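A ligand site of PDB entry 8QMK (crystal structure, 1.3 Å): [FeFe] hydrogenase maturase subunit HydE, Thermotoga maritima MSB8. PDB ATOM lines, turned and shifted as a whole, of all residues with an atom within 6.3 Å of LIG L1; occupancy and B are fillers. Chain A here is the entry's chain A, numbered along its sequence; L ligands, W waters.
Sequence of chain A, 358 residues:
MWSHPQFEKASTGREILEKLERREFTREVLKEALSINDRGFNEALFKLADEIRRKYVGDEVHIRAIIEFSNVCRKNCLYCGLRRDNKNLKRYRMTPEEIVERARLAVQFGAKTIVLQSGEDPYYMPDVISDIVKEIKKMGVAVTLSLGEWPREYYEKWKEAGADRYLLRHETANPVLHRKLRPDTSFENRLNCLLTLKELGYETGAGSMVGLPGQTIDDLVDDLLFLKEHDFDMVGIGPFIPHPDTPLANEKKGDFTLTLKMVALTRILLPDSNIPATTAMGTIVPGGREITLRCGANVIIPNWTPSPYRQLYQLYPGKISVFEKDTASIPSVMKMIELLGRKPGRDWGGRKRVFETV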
ATOM      1  N   VAL A  72      12.411 -16.966 -19.082  1.00  0.00           N
ATOM      2  CA  VAL A  72      12.937 -16.162 -20.185  1.00  0.00           C
ATOM      3  C   VAL A  72      14.135 -15.356 -19.674  1.00  0.00           C
ATOM      4  O   VAL A  72      14.041 -14.653 -18.650  1.00  0.00           O
ATOM      5  CB  VAL A  72      11.816 -15.227 -20.702  1.00  0.00           C
ATOM      6  CG1 VAL A  72      12.363 -14.198 -21.722  1.00  0.00           C
ATOM      7  CG2 VAL A  72      10.568 -16.005 -21.261  1.00  0.00           C
ATOM      8  N   CYS A  73      15.236 -15.358 -20.462  1.00  0.00           N
ATOM      9  CA  CYS A  73      16.422 -14.582 -20.070  1.00  0.00           C
ATOM     10  C   CYS A  73      17.038 -13.906 -21.312  1.00  0.00           C
ATOM     11  O   CYS A  73      17.269 -14.542 -22.324  1.00  0.00           O
ATOM     12  CB  CYS A  73      17.458 -15.422 -19.289  1.00  0.00           C
ATOM     13  SG  CYS A  73      18.691 -14.371 -18.540  1.00  0.00           S
ATOM     14  N   ARG A  74      17.409 -12.635 -21.147  1.00  0.00           N
ATOM     15  CA  ARG A  74      18.100 -11.902 -22.202  1.00  0.00           C
ATOM     16  C   ARG A  74      19.609 -12.174 -22.168  1.00  0.00           C
ATOM     17  O   ARG A  74      20.263 -11.819 -23.194  1.00  0.00           O
ATOM     18  CB  ARG A  74      17.836 -10.389 -22.043  1.00  0.00           C
ATOM     19  CG  ARG A  74      18.444  -9.762 -20.761  1.00  0.00           C
ATOM     20  CD  ARG A  74      18.042  -8.312 -20.591  1.00  0.00           C
ATOM     21  NE  ARG A  74      18.593  -7.854 -19.319  1.00  0.00           N
ATOM     22  CZ  ARG A  74      18.624  -6.576 -18.975  1.00  0.00           C
ATOM     23  NH1 ARG A  74      18.174  -5.616 -19.797  1.00  0.00           N
ATOM     24  NH2 ARG A  74      19.201  -6.238 -17.807  1.00  0.00           N
ATOM     25  N   LYS A  75      20.164 -12.783 -21.104  1.00  0.00           N
ATOM     26  CA  LYS A  75      21.593 -13.034 -21.042  1.00  0.00           C
ATOM     27  C   LYS A  75      21.939 -14.419 -21.550  1.00  0.00           C
ATOM     28  O   LYS A  75      21.054 -15.208 -21.967  1.00  0.00           O
ATOM     29  CB  LYS A  75      22.081 -12.796 -19.581  1.00  0.00           C
ATOM     30  CG  LYS A  75      22.287 -11.315 -19.363  1.00  0.00           C
ATOM     31  CD  LYS A  75      22.878 -11.104 -17.953  1.00  0.00           C
ATOM     32  CE  LYS A  75      23.375  -9.664 -17.689  1.00  0.00           C
ATOM     33  NZ  LYS A  75      22.403  -8.538 -18.007  1.00  0.00           N
ATOM     34  N   ASN A  76      23.248 -14.719 -21.569  1.00  0.00           N
ATOM     35  CA  ASN A  76      23.764 -15.930 -22.248  1.00  0.00           C
ATOM     36  C   ASN A  76      24.871 -16.599 -21.437  1.00  0.00           C
ATOM     37  O   ASN A  76      25.815 -17.143 -22.006  1.00  0.00           O
ATOM     38  CB  ASN A  76      24.272 -15.561 -23.665  1.00  0.00           C
ATOM     39  CG  ASN A  76      24.140 -16.686 -24.698  1.00  0.00           C
ATOM     40  OD1 ASN A  76      23.292 -17.569 -24.582  1.00  0.00           O
ATOM     41  ND2 ASN A  76      25.021 -16.669 -25.673  1.00  0.00           N
ATOM     42  N   CYS A  77      24.762 -16.597 -20.119  1.00  0.00           N
ATOM     43  CA  CYS A  77      25.777 -17.188 -19.251  1.00  0.00           C
ATOM     44  C   CYS A  77      26.104 -18.599 -19.694  1.00  0.00           C
ATOM     45  O   CYS A  77      25.201 -19.412 -19.938  1.00  0.00           O
ATOM     46  CB  CYS A  77      25.315 -17.150 -17.781  1.00  0.00           C
ATOM     47  SG  CYS A  77      24.787 -15.514 -17.210  1.00  0.00           S
ATOM     48  N   TYR A  79      27.180 -21.233 -18.247  1.00  0.00           N
ATOM     49  CA  TYR A  79      26.847 -22.380 -17.373  1.00  0.00           C
ATOM     50  C   TYR A  79      25.352 -22.687 -17.307  1.00  0.00           C
ATOM     51  O   TYR A  79      25.011 -23.789 -16.829  1.00  0.00           O
ATOM     52  CB  TYR A  79      27.409 -22.122 -15.935  1.00  0.00           C
ATOM     53  CG  TYR A  79      27.147 -20.720 -15.444  1.00  0.00           C
ATOM     54  CD1 TYR A  79      25.880 -20.342 -14.911  1.00  0.00           C
ATOM     55  CD2 TYR A  79      28.125 -19.727 -15.473  1.00  0.00           C
ATOM     56  CE1 TYR A  79      25.640 -19.044 -14.465  1.00  0.00           C
ATOM     57  CE2 TYR A  79      27.893 -18.432 -15.021  1.00  0.00           C
ATOM     58  CZ  TYR A  79      26.614 -18.119 -14.474  1.00  0.00           C
ATOM     59  OH  TYR A  79      26.445 -16.794 -14.039  1.00  0.00           O
ATOM     60  N   CYS A  80      24.490 -21.734 -17.714  1.00  0.00           N
ATOM     61  CA  CYS A  80      23.053 -21.806 -17.305  1.00  0.00           C
ATOM     62  C   CYS A  80      22.153 -22.350 -18.400  1.00  0.00           C
ATOM     63  O   CYS A  80      22.183 -21.861 -19.544  1.00  0.00           O
ATOM     64  CB  CYS A  80      22.663 -20.384 -16.956  1.00  0.00           C
ATOM     65  SG  CYS A  80      20.921 -20.293 -16.340  1.00  0.00           S
ATOM     66  N   GLY A  81      21.263 -23.285 -18.036  1.00  0.00           N
ATOM     67  CA  GLY A  81      20.315 -23.810 -18.990  1.00  0.00           C
ATOM     68  C   GLY A  81      19.333 -22.761 -19.519  1.00  0.00           C
ATOM     69  O   GLY A  81      18.746 -22.997 -20.601  1.00  0.00           O
ATOM     70  N   LEU A  82      19.143 -21.664 -18.848  1.00  0.00           N
ATOM     71  CA  LEU A  82      18.190 -20.635 -19.352  1.00  0.00           C
ATOM     72  C   LEU A  82      18.856 -19.644 -20.309  1.00  0.00           C
ATOM     73  O   LEU A  82      18.162 -18.758 -20.842  1.00  0.00           O
ATOM     74  CB  LEU A  82      17.547 -19.836 -18.172  1.00  0.00           C
ATOM     75  CG  LEU A  82      16.927 -20.730 -17.085  1.00  0.00           C
ATOM     76  CD1 LEU A  82      16.124 -19.756 -16.153  1.00  0.00           C
ATOM     77  CD2 LEU A  82      16.114 -21.855 -17.635  1.00  0.00           C
ATOM     78  N   ARG A  83      20.150 -19.817 -20.606  1.00  0.00           N
ATOM     79  CA  ARG A  83      20.821 -18.879 -21.489  1.00  0.00           C
ATOM     80  C   ARG A  83      20.026 -18.743 -22.794  1.00  0.00           C
ATOM     81  O   ARG A  83      19.458 -19.721 -23.322  1.00  0.00           O
ATOM     82  CB  ARG A  83      22.258 -19.382 -21.770  1.00  0.00           C
ATOM     83  CG  ARG A  83      22.362 -20.721 -22.519  1.00  0.00           C
ATOM     84  CD  ARG A  83      23.767 -21.305 -22.327  1.00  0.00           C
ATOM     85  NE  ARG A  83      24.843 -20.384 -22.632  1.00  0.00           N
ATOM     86  CZ  ARG A  83      25.355 -20.154 -23.839  1.00  0.00           C
ATOM     87  NH1 ARG A  83      25.036 -20.896 -24.915  1.00  0.00           N
ATOM     88  NH2 ARG A  83      26.334 -19.220 -23.962  1.00  0.00           N
ATOM     89  N   ARG A  84      20.030 -17.534 -23.354  1.00  0.00           N
ATOM     90  CA  ARG A  84      19.164 -17.302 -24.527  1.00  0.00           C
ATOM     91  C   ARG A  84      19.491 -18.218 -25.693  1.00  0.00           C
ATOM     92  O   ARG A  84      18.583 -18.499 -26.526  1.00  0.00           O
ATOM     93  CB  ARG A  84      19.187 -15.840 -24.988  1.00  0.00           C
ATOM     94  CG  ARG A  84      20.523 -15.409 -25.500  1.00  0.00           C
ATOM     95  CD  ARG A  84      20.507 -13.940 -25.971  1.00  0.00           C
ATOM     96  NE  ARG A  84      21.795 -13.589 -26.516  1.00  0.00           N
ATOM     97  CZ  ARG A  84      22.809 -13.023 -25.857  1.00  0.00           C
ATOM     98  NH1 ARG A  84      22.662 -12.487 -24.616  1.00  0.00           N
ATOM     99  NH2 ARG A  84      24.022 -13.003 -26.457  1.00  0.00           N
ATOM    100  N   SER A 118      13.679 -15.195 -11.420  1.00  0.00           N
ATOM    101  CA  SER A 118      13.406 -15.353 -12.831  1.00  0.00           C
ATOM    102  C   SER A 118      14.702 -15.251 -13.612  1.00  0.00           C
ATOM    103  O   SER A 118      15.715 -14.719 -13.138  1.00  0.00           O
ATOM    104  CB  SER A 118      12.403 -14.353 -13.323  1.00  0.00           C
ATOM    105  OG  SER A 118      12.847 -13.044 -13.212  1.00  0.00           O
ATOM    106  N   GLY A 119      14.648 -15.700 -14.872  1.00  0.00           N
ATOM    107  CA  GLY A 119      15.597 -15.150 -15.883  1.00  0.00           C
ATOM    108  C   GLY A 119      15.472 -13.626 -15.935  1.00  0.00           C
ATOM    109  O   GLY A 119      14.457 -13.027 -15.467  1.00  0.00           O
ATOM    110  N   GLU A 120      16.443 -12.955 -16.589  1.00  0.00           N
ATOM    111  CA  GLU A 120      16.311 -11.519 -16.817  1.00  0.00           C
ATOM    112  C   GLU A 120      15.307 -11.303 -17.958  1.00  0.00           C
ATOM    113  O   GLU A 120      15.664 -11.216 -19.157  1.00  0.00           O
ATOM    114  CB  GLU A 120      17.663 -10.889 -17.184  1.00  0.00           C
ATOM    115  CG  GLU A 120      18.639 -10.933 -15.977  1.00  0.00           C
ATOM    116  CD  GLU A 120      19.791  -9.966 -16.168  1.00  0.00           C
ATOM    117  OE1 GLU A 120      19.851  -9.240 -17.197  1.00  0.00           O
ATOM    118  OE2 GLU A 120      20.722  -9.998 -15.304  1.00  0.00           O
ATOM    119  N   GLY A 148      18.255 -10.576 -11.289  1.00  0.00           N
ATOM    120  CA  GLY A 148      19.459 -10.209 -12.058  1.00  0.00           C
ATOM    121  C   GLY A 148      19.803  -8.757 -11.976  1.00  0.00           C
ATOM    122  O   GLY A 148      19.501  -8.048 -11.015  1.00  0.00           O
ATOM    123  N   GLU A 171      28.785 -15.151  -8.283  1.00  0.00           N
ATOM    124  CA  GLU A 171      29.180 -16.225  -9.194  1.00  0.00           C
ATOM    125  C   GLU A 171      30.671 -16.589  -9.083  1.00  0.00           C
ATOM    126  O   GLU A 171      31.030 -17.735  -8.778  1.00  0.00           O
ATOM    127  CB  GLU A 171      28.794 -15.961 -10.702  1.00  0.00           C
ATOM    128  CG  GLU A 171      27.323 -15.375 -10.837  1.00  0.00           C
ATOM    129  CD  GLU A 171      26.236 -16.235 -10.290  1.00  0.00           C
ATOM    130  OE1 GLU A 171      26.450 -17.283  -9.674  1.00  0.00           O
ATOM    131  OE2 GLU A 171      25.061 -15.825 -10.535  1.00  0.00           O
ATOM    132  N   ARG A 182      30.255 -15.049 -18.443  1.00  0.00           N
ATOM    133  CA  ARG A 182      29.063 -14.171 -18.447  1.00  0.00           C
ATOM    134  C   ARG A 182      29.312 -13.076 -19.488  1.00  0.00           C
ATOM    135  O   ARG A 182      29.641 -11.920 -19.147  1.00  0.00           O
ATOM    136  CB  ARG A 182      28.769 -13.652 -17.049  1.00  0.00           C
ATOM    137  CG  ARG A 182      28.721 -14.727 -16.003  1.00  0.00           C
ATOM    138  CD  ARG A 182      28.247 -14.255 -14.638  1.00  0.00           C
ATOM    139  NE  ARG A 182      26.835 -13.904 -14.728  1.00  0.00           N
ATOM    140  CZ  ARG A 182      26.304 -12.686 -14.576  1.00  0.00           C
ATOM    141  NH1 ARG A 182      27.002 -11.645 -14.217  1.00  0.00           N
ATOM    142  NH2 ARG A 182      25.026 -12.517 -14.932  1.00  0.00           N
ATOM    143  N   ARG A 190      28.338  -6.492 -11.773  1.00  0.00           N
ATOM    144  CA  ARG A 190      27.675  -7.305 -10.742  1.00  0.00           C
ATOM    145  C   ARG A 190      27.893  -6.676  -9.360  1.00  0.00           C
ATOM    146  O   ARG A 190      26.962  -6.537  -8.524  1.00  0.00           O
ATOM    147  CB  ARG A 190      28.263  -8.737 -10.774  1.00  0.00           C
ATOM    148  CG  ARG A 190      27.422  -9.825 -10.011  1.00  0.00           C
ATOM    149  CD  ARG A 190      26.326 -10.192 -10.879  1.00  0.00           C
ATOM    150  NE  ARG A 190      25.658 -11.462 -10.430  1.00  0.00           N
ATOM    151  CZ  ARG A 190      24.521 -11.887 -10.991  1.00  0.00           C
ATOM    152  NH1 ARG A 190      23.986 -11.249 -12.013  1.00  0.00           N
ATOM    153  NH2 ARG A 190      23.874 -12.918 -10.432  1.00  0.00           N
ATOM    154  N   TYR A 313      12.102 -24.886 -15.389  1.00  0.00           N
ATOM    155  CA  TYR A 313      13.083 -23.910 -14.852  1.00  0.00           C
ATOM    156  C   TYR A 313      14.431 -24.620 -14.675  1.00  0.00           C
ATOM    157  O   TYR A 313      14.936 -24.843 -13.560  1.00  0.00           O
ATOM    158  CB  TYR A 313      12.549 -23.277 -13.561  1.00  0.00           C
ATOM    159  CG  TYR A 313      13.343 -22.043 -13.141  1.00  0.00           C
ATOM    160  CD1 TYR A 313      13.134 -20.786 -13.758  1.00  0.00           C
ATOM    161  CD2 TYR A 313      14.251 -22.128 -12.065  1.00  0.00           C
ATOM    162  CE1 TYR A 313      13.795 -19.646 -13.330  1.00  0.00           C
ATOM    163  CE2 TYR A 313      14.931 -21.014 -11.619  1.00  0.00           C
ATOM    164  CZ  TYR A 313      14.722 -19.758 -12.237  1.00  0.00           C
ATOM    165  OH  TYR A 313      15.349 -18.634 -11.773  1.00  0.00           O
ATOM    166  N   LEU A 315      17.807 -24.764 -14.723  1.00  0.00           N
ATOM    167  CA  LEU A 315      19.127 -24.126 -14.599  1.00  0.00           C
ATOM    168  C   LEU A 315      20.227 -25.149 -14.834  1.00  0.00           C
ATOM    169  O   LEU A 315      21.242 -24.858 -15.483  1.00  0.00           O
ATOM    170  CB  LEU A 315      19.317 -23.578 -13.180  1.00  0.00           C
ATOM    171  CG  LEU A 315      18.348 -22.556 -12.715  1.00  0.00           C
ATOM    172  CD1 LEU A 315      18.673 -22.172 -11.273  1.00  0.00           C
ATOM    173  CD2 LEU A 315      18.376 -21.254 -13.513  1.00  0.00           C
HETATM  174 FE1  LIG L   1      20.842 -17.987 -16.189  1.00  0.00          FE
HETATM  175 FE2  LIG L   1      20.002 -15.648 -17.239  1.00  0.00          FE
HETATM  176 FE3  LIG L   1      22.607 -15.943 -16.513  1.00  0.00          FE
HETATM  177 FE4  LIG L   1      20.581 -15.749 -14.425  1.00  0.00          FE
HETATM  178  S1  LIG L   1      21.308 -14.148 -16.058  1.00  0.00           S
HETATM  179  S2  LIG L   1      22.355 -17.265 -14.623  1.00  0.00           S
HETATM  180  S3  LIG L   1      18.925 -16.926 -15.675  1.00  0.00           S
HETATM  181  S4  LIG L   1      21.499 -17.050 -18.227  1.00  0.00           S
HETATM  182  N1  LG2 L   2      18.926 -14.423 -13.523  1.00  0.00           N
HETATM  183  C1  LG2 L   2      19.153 -14.229 -12.073  1.00  0.00           C
HETATM  184  C2  LG2 L   2      18.388 -15.282 -11.198  1.00  0.00           C
HETATM  185  C3  LG2 L   2      18.247 -16.672 -11.820  1.00  0.00           C
HETATM  186  S1  LG2 L   2      19.732 -17.630 -12.049  1.00  0.00           S
HETATM  187  C4  LG2 L   2      20.666 -14.195 -11.866  1.00  0.00           C
HETATM  188  O1  LG2 L   2      21.041 -13.750 -10.748  1.00  0.00           O
HETATM  189  O2  LG2 L   2      21.447 -14.713 -12.704  1.00  0.00           O
HETATM  190  C5  LG2 L   2      20.044 -18.060 -10.242  1.00  0.00           C
HETATM  191  C6  LG2 L   2      21.400 -18.737  -9.957  1.00  0.00           C
HETATM  192  O3  LG2 L   2      21.464 -20.070 -10.480  1.00  0.00           O
HETATM  193  C7  LG2 L   2      22.695 -18.057 -10.454  1.00  0.00           C
HETATM  194  O4  LG2 L   2      23.033 -16.991  -9.547  1.00  0.00           O
HETATM  195  C8  LG2 L   2      23.700 -19.196 -10.414  1.00  0.00           C
HETATM  196  O5  LG2 L   2      24.554 -19.191  -9.305  1.00  0.00           O
HETATM  197  C9  LG2 L   2      22.836 -20.495 -10.370  1.00  0.00           C
HETATM  198  N2  LG2 L   2      23.111 -21.420 -11.486  1.00  0.00           N
HETATM  199  C10 LG2 L   2      22.871 -21.156 -12.814  1.00  0.00           C
HETATM  200  N3  LG2 L   2      23.358 -22.163 -13.585  1.00  0.00           N
HETATM  201  C11 LG2 L   2      23.908 -23.102 -12.723  1.00  0.00           C
HETATM  202  C12 LG2 L   2      24.541 -24.305 -12.929  1.00  0.00           C
HETATM  203  N4  LG2 L   2      24.779 -24.893 -14.127  1.00  0.00           N
HETATM  204  N5  LG2 L   2      25.016 -24.968 -11.829  1.00  0.00           N
HETATM  205  C13 LG2 L   2      24.784 -24.468 -10.575  1.00  0.00           C
HETATM  206  N6  LG2 L   2      24.150 -23.300 -10.318  1.00  0.00           N
HETATM  207  C14 LG2 L   2      23.728 -22.592 -11.412  1.00  0.00           C
HETATM  208  O   HOH W   1      24.449 -15.243 -13.115  1.00  0.00           O
HETATM  209  O   HOH W   2      21.845 -11.908 -13.703  1.00  0.00           O
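CB of Lys 75 touches S1 of LIG L1, at 3.9 Å. Tyr 79 touches LIG L1 (CE1 to S2, 3.7 Å). CA of Arg 83 touches S4 of LIG L1, at 3.8 Å. CA of Gly 119 touches S3 of LIG L1 (3.8 Å). Seven residues have an atom within 4 Å of LIG L1: Cys 73, Lys 75, Cys 77, Tyr 79, Cys 80, Arg 83 and Gly 119. The nearest printed residue that does not touch LIG L1 is Leu 82 (4.01 Å).
SG of Cys 73 sits close to N of Lys 75 (3.4 Å). N of Glu 120 sits close to SG of Cys 73 (3.3 Å). The side-chain sulfur (SG) of Cys 80 lies close to the backbone NH (N) of Leu 82 (3.4 Å). The backbone carbonyl oxygen (O) of Cys 77 is in hydrogen-bond range of the guanidinium group (NE) of Arg 83 (2.9 Å). NE of Arg 182 lies close to SG of Cys 77, at 3.6 Å. OH of Tyr 79 sits at hydrogen-bond distance from NE of Arg 182. The guanidinium group (NH2) of Arg 83 sits at hydrogen-bond distance from the backbone carbonyl oxygen (O) of Asn 76 (2.9 Å). NZ of Lys 75 is in salt-bridge range of OE1 of Glu 120.
FE2 of LIG L1 is bound by SG of Cys 73 (2.2 Å). The side-chain sulfur of Cys 80 binds an iron atom (FE1) of LIG L1, 2.3 Å away. S4 of LIG L1 sits close to N of Cys 77, at 3.8 Å. FE3 of LIG L1 is bound by SG of Cys 77 (2.3 Å). A nitrogen (N4) of LG2 L2 sits at hydrogen-bond distance from the backbone carbonyl oxygen (O) of Tyr 79, at 2.9 Å. The backbone carbonyl oxygen of Ser 118 sits close to a nitrogen (N1) of LG2 L2, at 3.2 Å. The side-chain carboxylate (OE2) of Glu 171 sits at hydrogen-bond distance from an oxygen (O4) of LG2 L2 (2.5 Å). NH2 of Arg 190 is in salt-bridge range of O1 of LG2 L2 (3.0 Å).
Water W1 lies within hydrogen-bond range of the side-chain hydroxyl of Tyr 79, the side-chain carboxylate of Glu 171, the guanidinium group of Arg 182 and a sulfur (S2) of LIG L1. Water W2 lies within hydrogen-bond range of the side-chain carboxylate of Glu 120 (2.7 Å), the guanidinium group of Arg 190 (2.8 Å), a sulfur (S1) of LIG L1 (3.3 Å) and the guanidinium group of Arg 182 (3.5 Å).
O2 of LG2 L2 binds FE4 of LIG L1, 2.2 Å away.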
